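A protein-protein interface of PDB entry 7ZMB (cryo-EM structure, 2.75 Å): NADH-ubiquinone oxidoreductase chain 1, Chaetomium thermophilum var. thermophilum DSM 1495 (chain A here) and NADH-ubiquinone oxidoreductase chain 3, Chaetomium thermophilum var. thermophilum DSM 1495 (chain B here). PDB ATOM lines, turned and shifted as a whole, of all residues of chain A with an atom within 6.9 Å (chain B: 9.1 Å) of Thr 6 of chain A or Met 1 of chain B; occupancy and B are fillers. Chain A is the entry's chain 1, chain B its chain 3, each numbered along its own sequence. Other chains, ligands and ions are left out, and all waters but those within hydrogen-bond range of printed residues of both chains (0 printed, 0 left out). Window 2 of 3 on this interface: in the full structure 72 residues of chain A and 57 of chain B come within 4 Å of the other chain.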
ATOM      1  N   TYR A   3      32.806 -16.562  -9.695  1.00  0.00           N
ATOM      2  CA  TYR A   3      32.916 -15.472  -8.705  1.00  0.00           C
ATOM      3  C   TYR A   3      32.169 -15.860  -7.431  1.00  0.00           C
ATOM      4  O   TYR A   3      31.823 -17.033  -7.299  1.00  0.00           O
ATOM      5  CB  TYR A   3      32.494 -14.121  -9.285  1.00  0.00           C
ATOM      6  CG  TYR A   3      31.143 -14.054  -9.951  1.00  0.00           C
ATOM      7  CD1 TYR A   3      30.960 -14.484 -11.254  1.00  0.00           C
ATOM      8  CD2 TYR A   3      30.058 -13.501  -9.294  1.00  0.00           C
ATOM      9  CE1 TYR A   3      29.725 -14.400 -11.872  1.00  0.00           C
ATOM     10  CE2 TYR A   3      28.821 -13.405  -9.901  1.00  0.00           C
ATOM     11  CZ  TYR A   3      28.649 -13.861 -11.193  1.00  0.00           C
ATOM     12  OH  TYR A   3      27.427 -13.771 -11.790  1.00  0.00           O
ATOM     13  N   SER A   4      31.915 -14.885  -6.553  1.00  0.00           N
ATOM     14  CA  SER A   4      31.294 -15.143  -5.262  1.00  0.00           C
ATOM     15  C   SER A   4      29.831 -15.544  -5.402  1.00  0.00           C
ATOM     16  O   SER A   4      29.118 -15.095  -6.300  1.00  0.00           O
ATOM     17  CB  SER A   4      31.405 -13.902  -4.378  1.00  0.00           C
ATOM     18  OG  SER A   4      30.549 -13.994  -3.264  1.00  0.00           O
ATOM     19  N   GLN A   5      29.392 -16.412  -4.487  1.00  0.00           N
ATOM     20  CA  GLN A   5      27.977 -16.733  -4.359  1.00  0.00           C
ATOM     21  C   GLN A   5      27.153 -15.501  -4.019  1.00  0.00           C
ATOM     22  O   GLN A   5      26.078 -15.288  -4.590  1.00  0.00           O
ATOM     23  CB  GLN A   5      27.780 -17.800  -3.282  1.00  0.00           C
ATOM     24  CG  GLN A   5      26.499 -18.625  -3.384  1.00  0.00           C
ATOM     25  CD  GLN A   5      26.219 -19.177  -4.766  1.00  0.00           C
ATOM     26  OE1 GLN A   5      27.122 -19.351  -5.578  1.00  0.00           O
ATOM     27  NE2 GLN A   5      24.950 -19.454  -5.040  1.00  0.00           N
ATOM     28  N   THR A   6      27.623 -14.693  -3.072  1.00  0.00           N
ATOM     29  CA  THR A   6      26.823 -13.565  -2.616  1.00  0.00           C
ATOM     30  C   THR A   6      26.674 -12.511  -3.701  1.00  0.00           C
ATOM     31  O   THR A   6      25.612 -11.891  -3.818  1.00  0.00           O
ATOM     32  CB  THR A   6      27.436 -12.968  -1.352  1.00  0.00           C
ATOM     33  OG1 THR A   6      27.467 -13.967  -0.331  1.00  0.00           O
ATOM     34  CG2 THR A   6      26.615 -11.801  -0.858  1.00  0.00           C
ATOM     35  N   ILE A   7      27.713 -12.309  -4.513  1.00  0.00           N
ATOM     36  CA  ILE A   7      27.621 -11.321  -5.579  1.00  0.00           C
ATOM     37  C   ILE A   7      26.674 -11.794  -6.671  1.00  0.00           C
ATOM     38  O   ILE A   7      25.860 -11.017  -7.180  1.00  0.00           O
ATOM     39  CB  ILE A   7      29.017 -10.996  -6.131  1.00  0.00           C
ATOM     40  CG1 ILE A   7      29.899 -10.460  -5.014  1.00  0.00           C
ATOM     41  CG2 ILE A   7      28.922  -9.978  -7.248  1.00  0.00           C
ATOM     42  CD1 ILE A   7      29.373  -9.197  -4.402  1.00  0.00           C
ATOM     43  N   ASN A   8      26.764 -13.070  -7.054  1.00  0.00           N
ATOM     44  CA  ASN A   8      25.854 -13.600  -8.063  1.00  0.00           C
ATOM     45  C   ASN A   8      24.415 -13.471  -7.599  1.00  0.00           C
ATOM     46  O   ASN A   8      23.546 -13.023  -8.348  1.00  0.00           O
ATOM     47  CB  ASN A   8      26.200 -15.061  -8.363  1.00  0.00           C
ATOM     48  CG  ASN A   8      25.192 -15.729  -9.284  1.00  0.00           C
ATOM     49  OD1 ASN A   8      24.320 -16.466  -8.835  1.00  0.00           O
ATOM     50  ND2 ASN A   8      25.319 -15.485 -10.579  1.00  0.00           N
ATOM     51  N   SER A   9      24.157 -13.833  -6.345  1.00  0.00           N
ATOM     52  CA  SER A   9      22.839 -13.643  -5.757  1.00  0.00           C
ATOM     53  C   SER A   9      22.453 -12.173  -5.716  1.00  0.00           C
ATOM     54  O   SER A   9      21.286 -11.824  -5.920  1.00  0.00           O
ATOM     55  CB  SER A   9      22.823 -14.241  -4.355  1.00  0.00           C
ATOM     56  OG  SER A   9      21.709 -13.776  -3.631  1.00  0.00           O
ATOM     57  N   LEU A  10      23.420 -11.300  -5.436  1.00  0.00           N
ATOM     58  CA  LEU A  10      23.149  -9.871  -5.341  1.00  0.00           C
ATOM     59  C   LEU A  10      22.669  -9.310  -6.670  1.00  0.00           C
ATOM     60  O   LEU A  10      21.613  -8.674  -6.745  1.00  0.00           O
ATOM     61  CB  LEU A  10      24.411  -9.144  -4.873  1.00  0.00           C
ATOM     62  CG  LEU A  10      24.484  -7.626  -5.000  1.00  0.00           C
ATOM     63  CD1 LEU A  10      23.434  -6.957  -4.143  1.00  0.00           C
ATOM     64  CD2 LEU A  10      25.871  -7.143  -4.624  1.00  0.00           C
ATOM     65  N   VAL A  11      23.430  -9.546  -7.739  1.00  0.00           N
ATOM     66  CA  VAL A  11      23.108  -8.896  -9.003  1.00  0.00           C
ATOM     67  C   VAL A  11      21.874  -9.521  -9.635  1.00  0.00           C
ATOM     68  O   VAL A  11      21.140  -8.849 -10.362  1.00  0.00           O
ATOM     69  CB  VAL A  11      24.317  -8.924  -9.955  1.00  0.00           C
ATOM     70  CG1 VAL A  11      25.555  -8.425  -9.240  1.00  0.00           C
ATOM     71  CG2 VAL A  11      24.540 -10.312 -10.504  1.00  0.00           C
ATOM     72  N   MET B   1      25.790 -16.509  -0.443  1.00  0.00           N
ATOM     73  CA  MET B   1      24.470 -16.693   0.156  1.00  0.00           C
ATOM     74  C   MET B   1      23.424 -16.693  -0.971  1.00  0.00           C
ATOM     75  O   MET B   1      23.702 -16.207  -2.061  1.00  0.00           O
ATOM     76  CB  MET B   1      24.227 -15.608   1.214  1.00  0.00           C
ATOM     77  CG  MET B   1      22.823 -15.449   1.705  1.00  0.00           C
ATOM     78  SD  MET B   1      22.686 -14.268   3.064  1.00  0.00           S
ATOM     79  CE  MET B   1      23.551 -12.849   2.406  1.00  0.00           C
ATOM     80  N   SER B   2      22.250 -17.271  -0.726  1.00  0.00           N
ATOM     81  CA  SER B   2      21.336 -17.634  -1.800  1.00  0.00           C
ATOM     82  C   SER B   2      20.496 -16.454  -2.268  1.00  0.00           C
ATOM     83  O   SER B   2      20.183 -15.543  -1.502  1.00  0.00           O
ATOM     84  CB  SER B   2      20.402 -18.755  -1.355  1.00  0.00           C
ATOM     85  OG  SER B   2      19.449 -18.277  -0.428  1.00  0.00           O
ATOM     86  N   ALA B   3      20.080 -16.519  -3.533  1.00  0.00           N
ATOM     87  CA  ALA B   3      19.316 -15.431  -4.131  1.00  0.00           C
ATOM     88  C   ALA B   3      18.028 -15.164  -3.372  1.00  0.00           C
ATOM     89  O   ALA B   3      17.620 -14.010  -3.216  1.00  0.00           O
ATOM     90  CB  ALA B   3      19.020 -15.743  -5.597  1.00  0.00           C
ATOM     91  N   MET B   4      17.377 -16.220  -2.890  1.00  0.00           N
ATOM     92  CA  MET B   4      16.123 -16.056  -2.171  1.00  0.00           C
ATOM     93  C   MET B   4      16.314 -15.267  -0.882  1.00  0.00           C
ATOM     94  O   MET B   4      15.506 -14.390  -0.558  1.00  0.00           O
ATOM     95  CB  MET B   4      15.517 -17.426  -1.884  1.00  0.00           C
ATOM     96  CG  MET B   4      14.154 -17.344  -1.285  1.00  0.00           C
ATOM     97  SD  MET B   4      13.003 -16.643  -2.459  1.00  0.00           S
ATOM     98  CE  MET B   4      11.773 -16.012  -1.335  1.00  0.00           C
ATOM     99  N   SER B   5      17.372 -15.567  -0.132  1.00  0.00           N
ATOM    100  CA  SER B   5      17.597 -14.902   1.147  1.00  0.00           C
ATOM    101  C   SER B   5      17.846 -13.409   0.966  1.00  0.00           C
ATOM    102  O   SER B   5      17.277 -12.587   1.689  1.00  0.00           O
ATOM    103  CB  SER B   5      18.761 -15.571   1.873  1.00  0.00           C
ATOM    104  OG  SER B   5      19.834 -15.820   0.985  1.00  0.00           O
ATOM    105  N   ILE B   6      18.699 -13.036   0.005  1.00  0.00           N
ATOM    106  CA  ILE B   6      18.887 -11.624  -0.325  1.00  0.00           C
ATOM    107  C   ILE B   6      17.630 -11.000  -0.911  1.00  0.00           C
ATOM    108  O   ILE B   6      17.349  -9.824  -0.652  1.00  0.00           O
ATOM    109  CB  ILE B   6      20.119 -11.413  -1.243  1.00  0.00           C
ATOM    110  CG1 ILE B   6      21.417 -11.802  -0.529  1.00  0.00           C
ATOM    111  CG2 ILE B   6      20.172 -10.024  -1.836  1.00  0.00           C
ATOM    112  CD1 ILE B   6      21.821 -13.200  -0.656  1.00  0.00           C
ATOM    113  N   TYR B   7      16.847 -11.749  -1.690  1.00  0.00           N
ATOM    114  CA  TYR B   7      15.620 -11.171  -2.226  1.00  0.00           C
ATOM    115  C   TYR B   7      14.703 -10.715  -1.103  1.00  0.00           C
ATOM    116  O   TYR B   7      14.151  -9.612  -1.150  1.00  0.00           O
ATOM    117  CB  TYR B   7      14.902 -12.172  -3.129  1.00  0.00           C
ATOM    118  CG  TYR B   7      13.725 -11.593  -3.893  1.00  0.00           C
ATOM    119  CD1 TYR B   7      12.462 -11.540  -3.330  1.00  0.00           C
ATOM    120  CD2 TYR B   7      13.884 -11.105  -5.179  1.00  0.00           C
ATOM    121  CE1 TYR B   7      11.391 -11.017  -4.025  1.00  0.00           C
ATOM    122  CE2 TYR B   7      12.821 -10.584  -5.880  1.00  0.00           C
ATOM    123  CZ  TYR B   7      11.577 -10.543  -5.300  1.00  0.00           C
ATOM    124  OH  TYR B   7      10.511 -10.020  -5.990  1.00  0.00           O
ATOM    125  N   ILE B   9      15.608  -9.841   1.865  1.00  0.00           N
ATOM    126  CA  ILE B   9      16.208  -8.692   2.534  1.00  0.00           C
ATOM    127  C   ILE B   9      15.922  -7.417   1.756  1.00  0.00           C
ATOM    128  O   ILE B   9      15.485  -6.412   2.323  1.00  0.00           O
ATOM    129  CB  ILE B   9      17.718  -8.910   2.724  1.00  0.00           C
ATOM    130  CG1 ILE B   9      17.974 -10.172   3.538  1.00  0.00           C
ATOM    131  CG2 ILE B   9      18.342  -7.707   3.410  1.00  0.00           C
ATOM    132  CD1 ILE B   9      19.399 -10.645   3.482  1.00  0.00           C
ATOM    133  N   PHE B  10      16.147  -7.443   0.443  1.00  0.00           N
ATOM    134  CA  PHE B  10      15.993  -6.225  -0.344  1.00  0.00           C
ATOM    135  C   PHE B  10      14.554  -5.734  -0.363  1.00  0.00           C
ATOM    136  O   PHE B  10      14.310  -4.530  -0.282  1.00  0.00           O
ATOM    137  CB  PHE B  10      16.511  -6.418  -1.767  1.00  0.00           C
ATOM    138  CG  PHE B  10      18.002  -6.444  -1.860  1.00  0.00           C
ATOM    139  CD1 PHE B  10      18.778  -6.064  -0.777  1.00  0.00           C
ATOM    140  CD2 PHE B  10      18.633  -6.799  -3.033  1.00  0.00           C
ATOM    141  CE1 PHE B  10      20.154  -6.073  -0.857  1.00  0.00           C
ATOM    142  CE2 PHE B  10      20.007  -6.808  -3.121  1.00  0.00           C
ATOM    143  CZ  PHE B  10      20.769  -6.444  -2.029  1.00  0.00           C
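Printed residues of chain A that touch a printed residue of chain B: Gln 5, Thr 6, Ser 9 and Leu 10.
Hydrophobic or aromatic side chains of chain A within 4 Å of the printed part of chain B: Leu 10.
Printed residues of chain B that touch a printed residue of chain A: Met 1, Ser 2, Ala 3, Ile 6 and Phe 10.
Hydrophobic or aromatic side chains of chain B that line the printed part of chain A: Met 1, Ala 3, Ile 6 and Phe 10.
Among the printed residues, 7 pairs touch across the chains.
Among the printed residues, no Asp or Glu carboxylate lies within 4 Å of a Lys or Arg side-chain nitrogen of the other chain.
Gln 5 of chain A touches Met 1 of chain B (O to O, 3.6 Å).
Ser 9 of chain A touches Met 1 of chain B (CB to O, 3.1 Å).
Ile 6 of chain B touches Ser 9 of chain A (CD1 to OG, 3.0 Å).
CD1 of Leu 10 of chain A touches CZ of Phe 10 of chain B (3.4 Å).
Thr 6 of chain A touches one residue of chain B.
No residue of chain B comes within 4 Å of Ile 7 of chain A.
Of the printed residues of chain A, Met 1 of chain B touches Gln 5, Thr 6 and Ser 9.
Ser 5 of chain B touches none of the printed residues of chain A.
Of the printed residues of chain A, Ile 6 of chain B touches Ser 9.
Ile 9 of chain B touches none of the printed residues of chain A.
Of the printed residues of chain A, Phe 10 of chain B touches Leu 10.
The nearest residue of chain A that does not touch Met 1 of chain B is Leu 10 of chain A (6.0 Å).
The nearest printed residue of chain A that does not touch Ser 2 of chain B is Gln 5 of chain A (5.2 Å).
OG of Ser 5 of chain B lies within hydrogen-bond range of O of Ser 2 of chain B (2.5 Å).
The side-chain hydroxyl (OG) of Ser 4 of chain A is in hydrogen-bond range of the backbone NH (N) of Thr 6 of chain A.
OG of Ser 9 of chain A lies close to N of Ala 3 of chain B (3.2 Å).
The backbone carbonyl oxygen (O) of Ser 2 of chain B sits at hydrogen-bond distance from the side-chain hydroxyl (OG) of Ser 9 of chain A.
The side-chain hydroxyl (OG1) of Thr 6 of chain A sits at hydrogen-bond distance from the backbone NH (N) of Met 1 of chain B, at 3.0 Å.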
